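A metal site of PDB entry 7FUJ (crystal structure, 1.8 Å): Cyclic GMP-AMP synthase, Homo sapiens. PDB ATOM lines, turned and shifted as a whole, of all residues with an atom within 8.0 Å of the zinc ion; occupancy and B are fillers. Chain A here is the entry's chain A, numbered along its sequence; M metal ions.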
ATOM      1  N   LEU A 227     -14.437  -4.933 -17.107  1.00  0.00           N
ATOM      2  CA  LEU A 227     -14.916  -4.297 -15.866  1.00  0.00           C
ATOM      3  C   LEU A 227     -13.740  -3.804 -15.017  1.00  0.00           C
ATOM      4  O   LEU A 227     -13.888  -2.750 -14.360  1.00  0.00           O
ATOM      5  CB  LEU A 227     -15.830  -5.276 -15.129  1.00  0.00           C
ATOM      6  CG  LEU A 227     -17.264  -5.228 -15.616  1.00  0.00           C
ATOM      7  CD1 LEU A 227     -18.116  -6.349 -15.040  1.00  0.00           C
ATOM      8  CD2 LEU A 227     -17.874  -3.864 -15.321  1.00  0.00           C
ATOM      9  N   ASN A 229     -10.838  -2.848 -16.223  1.00  0.00           N
ATOM     10  CA  ASN A 229     -10.020  -1.898 -17.037  1.00  0.00           C
ATOM     11  C   ASN A 229     -10.980  -1.186 -17.992  1.00  0.00           C
ATOM     12  O   ASN A 229     -10.967  -1.510 -19.193  1.00  0.00           O
ATOM     13  CB  ASN A 229      -8.875  -2.633 -17.723  1.00  0.00           C
ATOM     14  CG  ASN A 229      -7.841  -1.722 -18.358  1.00  0.00           C
ATOM     15  OD1 ASN A 229      -7.907  -0.498 -18.232  1.00  0.00           O
ATOM     16  ND2 ASN A 229      -6.872  -2.318 -18.993  1.00  0.00           N
ATOM     17  N   HIS A 230     -11.843  -0.326 -17.431  1.00  0.00           N
ATOM     18  CA  HIS A 230     -13.180  -0.008 -17.973  1.00  0.00           C
ATOM     19  C   HIS A 230     -13.243   1.406 -18.547  1.00  0.00           C
ATOM     20  O   HIS A 230     -14.344   1.782 -18.994  1.00  0.00           O
ATOM     21  CB  HIS A 230     -14.264  -0.172 -16.877  1.00  0.00           C
ATOM     22  CG  HIS A 230     -14.002   0.707 -15.715  1.00  0.00           C
ATOM     23  ND1 HIS A 230     -13.580   0.228 -14.480  1.00  0.00           N
ATOM     24  CD2 HIS A 230     -13.970   2.063 -15.643  1.00  0.00           C
ATOM     25  CE1 HIS A 230     -13.335   1.266 -13.691  1.00  0.00           C
ATOM     26  NE2 HIS A 230     -13.545   2.390 -14.389  1.00  0.00           N
ATOM     27  N   GLY A 231     -12.160   2.188 -18.498  1.00  0.00           N
ATOM     28  CA  GLY A 231     -12.205   3.612 -18.917  1.00  0.00           C
ATOM     29  C   GLY A 231     -11.660   3.834 -20.333  1.00  0.00           C
ATOM     30  O   GLY A 231     -10.826   3.033 -20.777  1.00  0.00           O
ATOM     31  N   LYS A 232     -12.038   4.939 -20.980  1.00  0.00           N
ATOM     32  CA  LYS A 232     -11.265   5.391 -22.161  1.00  0.00           C
ATOM     33  C   LYS A 232      -9.866   5.798 -21.689  1.00  0.00           C
ATOM     34  O   LYS A 232      -8.859   5.417 -22.353  1.00  0.00           O
ATOM     35  CB  LYS A 232     -11.974   6.531 -22.886  1.00  0.00           C
ATOM     36  CG  LYS A 232     -11.115   7.157 -23.971  1.00  0.00           C
ATOM     37  CD  LYS A 232     -11.823   8.177 -24.831  1.00  0.00           C
ATOM     38  CE  LYS A 232     -12.967   7.609 -25.639  1.00  0.00           C
ATOM     39  NZ  LYS A 232     -12.495   6.609 -26.620  1.00  0.00           N
ATOM     40  N   SER A 233      -9.762   6.527 -20.569  1.00  0.00           N
ATOM     41  CA  SER A 233      -8.458   6.874 -19.967  1.00  0.00           C
ATOM     42  C   SER A 233      -7.870   5.621 -19.329  1.00  0.00           C
ATOM     43  O   SER A 233      -8.578   4.924 -18.558  1.00  0.00           O
ATOM     44  CB  SER A 233      -8.532   7.961 -18.963  1.00  0.00           C
ATOM     45  OG  SER A 233      -7.266   8.113 -18.350  1.00  0.00           O
ATOM     46  N   THR A 235      -5.940   5.653 -16.947  1.00  0.00           N
ATOM     47  CA  THR A 235      -5.871   5.952 -15.490  1.00  0.00           C
ATOM     48  C   THR A 235      -7.283   6.131 -14.911  1.00  0.00           C
ATOM     49  O   THR A 235      -7.407   6.631 -13.781  1.00  0.00           O
ATOM     50  CB  THR A 235      -4.919   7.123 -15.200  1.00  0.00           C
ATOM     51  OG1 THR A 235      -5.263   8.287 -15.965  1.00  0.00           O
ATOM     52  CG2 THR A 235      -3.492   6.747 -15.519  1.00  0.00           C
ATOM     53  N   CYS A 236      -8.338   5.728 -15.623  1.00  0.00           N
ATOM     54  CA  CYS A 236      -9.710   5.804 -15.058  1.00  0.00           C
ATOM     55  C   CYS A 236      -9.711   5.159 -13.675  1.00  0.00           C
ATOM     56  O   CYS A 236      -9.236   4.059 -13.568  1.00  0.00           O
ATOM     57  CB  CYS A 236     -10.744   5.118 -15.935  1.00  0.00           C
ATOM     58  SG  CYS A 236     -12.423   5.635 -15.515  1.00  0.00           S
ATOM     59  N   CYS A 237     -10.213   5.871 -12.652  1.00  0.00           N
ATOM     60  CA  CYS A 237     -10.379   5.401 -11.251  1.00  0.00           C
ATOM     61  C   CYS A 237      -9.049   5.126 -10.546  1.00  0.00           C
ATOM     62  O   CYS A 237      -9.093   4.585  -9.446  1.00  0.00           O
ATOM     63  CB  CYS A 237     -11.282   4.169 -11.196  1.00  0.00           C
ATOM     64  SG  CYS A 237     -12.994   4.604 -11.615  1.00  0.00           S
ATOM     65  N   GLU A 238      -7.903   5.512 -11.132  1.00  0.00           N
ATOM     66  CA  GLU A 238      -6.607   5.354 -10.441  1.00  0.00           C
ATOM     67  C   GLU A 238      -6.302   6.591  -9.603  1.00  0.00           C
ATOM     68  O   GLU A 238      -5.362   6.518  -8.873  1.00  0.00           O
ATOM     69  CB  GLU A 238      -5.468   5.108 -11.435  1.00  0.00           C
ATOM     70  CG  GLU A 238      -5.439   3.688 -11.953  1.00  0.00           C
ATOM     71  CD  GLU A 238      -4.111   3.281 -12.583  1.00  0.00           C
ATOM     72  OE1 GLU A 238      -3.261   4.172 -12.792  1.00  0.00           O
ATOM     73  OE2 GLU A 238      -3.924   2.063 -12.830  1.00  0.00           O
ATOM     74  N   ASN A 239      -7.025   7.703  -9.775  1.00  0.00           N
ATOM     75  CA  ASN A 239      -6.752   8.988  -9.077  1.00  0.00           C
ATOM     76  C   ASN A 239      -8.092   9.693  -8.807  1.00  0.00           C
ATOM     77  O   ASN A 239      -9.123   9.292  -9.374  1.00  0.00           O
ATOM     78  CB  ASN A 239      -5.784   9.882  -9.852  1.00  0.00           C
ATOM     79  CG  ASN A 239      -6.319  10.295 -11.207  1.00  0.00           C
ATOM     80  OD1 ASN A 239      -7.223  11.138 -11.309  1.00  0.00           O
ATOM     81  ND2 ASN A 239      -5.773   9.727 -12.268  1.00  0.00           N
ATOM     82  N   GLU A 242     -10.304  11.267 -11.612  1.00  0.00           N
ATOM     83  CA  GLU A 242     -10.857  10.322 -12.621  1.00  0.00           C
ATOM     84  C   GLU A 242     -11.627   9.193 -11.926  1.00  0.00           C
ATOM     85  O   GLU A 242     -11.503   8.046 -12.340  1.00  0.00           O
ATOM     86  CB  GLU A 242      -9.761   9.717 -13.504  1.00  0.00           C
ATOM     87  CG  GLU A 242      -8.920  10.715 -14.272  1.00  0.00           C
ATOM     88  CD  GLU A 242      -7.891  10.045 -15.185  1.00  0.00           C
ATOM     89  OE1 GLU A 242      -8.281   9.575 -16.282  1.00  0.00           O
ATOM     90  OE2 GLU A 242      -6.714  10.007 -14.799  1.00  0.00           O
ATOM     91  N   LYS A 243     -12.481   9.518 -10.958  1.00  0.00           N
ATOM     92  CA  LYS A 243     -13.391   8.513 -10.329  1.00  0.00           C
ATOM     93  C   LYS A 243     -14.686   8.529 -11.137  1.00  0.00           C
ATOM     94  O   LYS A 243     -15.417   9.519 -11.024  1.00  0.00           O
ATOM     95  CB  LYS A 243     -13.610   8.849  -8.852  1.00  0.00           C
ATOM     96  CG  LYS A 243     -12.366   8.717  -7.983  1.00  0.00           C
ATOM     97  CD  LYS A 243     -11.851   7.291  -7.872  1.00  0.00           C
ATOM     98  CE  LYS A 243     -10.511   7.190  -7.169  1.00  0.00           C
ATOM     99  NZ  LYS A 243     -10.129   5.776  -6.949  1.00  0.00           N
ATOM    100  N   CYS A 244     -14.913   7.522 -12.001  1.00  0.00           N
ATOM    101  CA  CYS A 244     -16.140   7.391 -12.799  1.00  0.00           C
ATOM    102  C   CYS A 244     -17.156   6.614 -11.936  1.00  0.00           C
ATOM    103  O   CYS A 244     -16.754   6.103 -10.861  1.00  0.00           O
ATOM    104  CB  CYS A 244     -15.874   6.792 -14.165  1.00  0.00           C
ATOM    105  SG  CYS A 244     -15.717   4.979 -14.153  1.00  0.00           S
ATOM    106  N   CYS A 245     -18.408   6.606 -12.353  1.00  0.00           N
ATOM    107  CA  CYS A 245     -19.537   5.955 -11.633  1.00  0.00           C
ATOM    108  C   CYS A 245     -20.038   4.732 -12.436  1.00  0.00           C
ATOM    109  O   CYS A 245     -21.145   4.235 -12.162  1.00  0.00           O
ATOM    110  CB  CYS A 245     -20.628   6.980 -11.330  1.00  0.00           C
ATOM    111  SG  CYS A 245     -21.497   7.556 -12.807  1.00  0.00           S
ATOM    112  N   ARG A 246     -19.202   4.141 -13.292  1.00  0.00           N
ATOM    113  CA  ARG A 246     -19.569   2.944 -14.091  1.00  0.00           C
ATOM    114  C   ARG A 246     -19.940   1.775 -13.170  1.00  0.00           C
ATOM    115  O   ARG A 246     -21.070   1.277 -13.285  1.00  0.00           O
ATOM    116  CB  ARG A 246     -18.479   2.543 -15.081  1.00  0.00           C
ATOM    117  CG  ARG A 246     -18.409   3.459 -16.295  1.00  0.00           C
ATOM    118  CD  ARG A 246     -17.398   2.902 -17.261  1.00  0.00           C
ATOM    119  NE  ARG A 246     -17.180   3.648 -18.476  1.00  0.00           N
ATOM    120  CZ  ARG A 246     -16.294   4.633 -18.595  1.00  0.00           C
ATOM    121  NH1 ARG A 246     -16.113   5.184 -19.777  1.00  0.00           N
ATOM    122  NH2 ARG A 246     -15.534   5.003 -17.567  1.00  0.00           N
ATOM    123  N   LYS A 247     -19.040   1.373 -12.270  1.00  0.00           N
ATOM    124  CA  LYS A 247     -19.284   0.199 -11.416  1.00  0.00           C
ATOM    125  C   LYS A 247     -20.413   0.512 -10.420  1.00  0.00           C
ATOM    126  O   LYS A 247     -21.202  -0.395 -10.088  1.00  0.00           O
ATOM    127  CB  LYS A 247     -17.973  -0.249 -10.776  1.00  0.00           C
ATOM    128  CG  LYS A 247     -16.990  -0.901 -11.733  1.00  0.00           C
ATOM    129  CD  LYS A 247     -15.820  -1.540 -11.019  1.00  0.00           C
ATOM    130  CE  LYS A 247     -15.098  -2.553 -11.880  1.00  0.00           C
ATOM    131  NZ  LYS A 247     -13.976  -3.208 -11.173  1.00  0.00           N
ATOM    132  N   ASP A 292     -15.382   8.917 -20.676  1.00  0.00           N
ATOM    133  CA  ASP A 292     -15.361   8.902 -19.198  1.00  0.00           C
ATOM    134  C   ASP A 292     -16.162  10.105 -18.692  1.00  0.00           C
ATOM    135  O   ASP A 292     -16.737   9.992 -17.598  1.00  0.00           O
ATOM    136  CB  ASP A 292     -13.943   8.908 -18.624  1.00  0.00           C
ATOM    137  CG  ASP A 292     -13.103   7.704 -19.022  1.00  0.00           C
ATOM    138  OD1 ASP A 292     -13.715   6.656 -19.377  1.00  0.00           O
ATOM    139  OD2 ASP A 292     -11.873   7.839 -19.027  1.00  0.00           O
ATOM    140  N   TRP A 295     -19.676   9.537 -17.481  1.00  0.00           N
ATOM    141  CA  TRP A 295     -19.786   8.712 -16.244  1.00  0.00           C
ATOM    142  C   TRP A 295     -19.155   9.456 -15.082  1.00  0.00           C
ATOM    143  O   TRP A 295     -18.514   8.827 -14.247  1.00  0.00           O
ATOM    144  CB  TRP A 295     -19.130   7.318 -16.455  1.00  0.00           C
ATOM    145  CG  TRP A 295     -19.780   6.512 -17.537  1.00  0.00           C
ATOM    146  CD1 TRP A 295     -19.406   6.425 -18.842  1.00  0.00           C
ATOM    147  CD2 TRP A 295     -20.933   5.665 -17.395  1.00  0.00           C
ATOM    148  NE1 TRP A 295     -20.237   5.580 -19.520  1.00  0.00           N
ATOM    149  CE2 TRP A 295     -21.190   5.111 -18.653  1.00  0.00           C
ATOM    150  CE3 TRP A 295     -21.770   5.324 -16.323  1.00  0.00           C
ATOM    151  CZ2 TRP A 295     -22.242   4.220 -18.868  1.00  0.00           C
ATOM    152  CZ3 TRP A 295     -22.817   4.467 -16.552  1.00  0.00           C
ATOM    153  CH2 TRP A 295     -23.041   3.903 -17.802  1.00  0.00           C
HETATM  154 ZN    ZN M   1     -13.441   4.439 -13.837  1.00  0.00          ZN
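Four residues have an atom within 4 Å of the zinc ion: His 230, Cys 236, Cys 237 and Cys 244.
The zinc ion is bound by a ring nitrogen (NE2) of His 230 (2.1 Å), the side-chain sulfur of Cys 237 (2.3 Å), the side-chain sulfur of Cys 236 (2.3 Å) and the side-chain sulfur of Cys 244 (2.4 Å). The zinc ion has four donor atoms within binding distance.
The backbone carbonyl oxygen of His 230 is in hydrogen-bond range of the guanidinium group of Arg 246. The backbone carbonyl oxygen (O) of Leu 227 is in hydrogen-bond range of a ring nitrogen (ND1) of His 230 (3.0 Å). O of Glu 242 is in hydrogen-bond range of N of Cys 237. The backbone carbonyl oxygen of Cys 237 lies within hydrogen-bond range of the side-chain amino group of Lys 243. The guanidinium group (NH2) of Arg 246 sits close to the side-chain sulfur (SG) of Cys 236 (3.8 Å). The side-chain sulfur (SG) of Cys 244 sits close to the guanidinium group (NH2) of Arg 246, at 3.4 Å.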
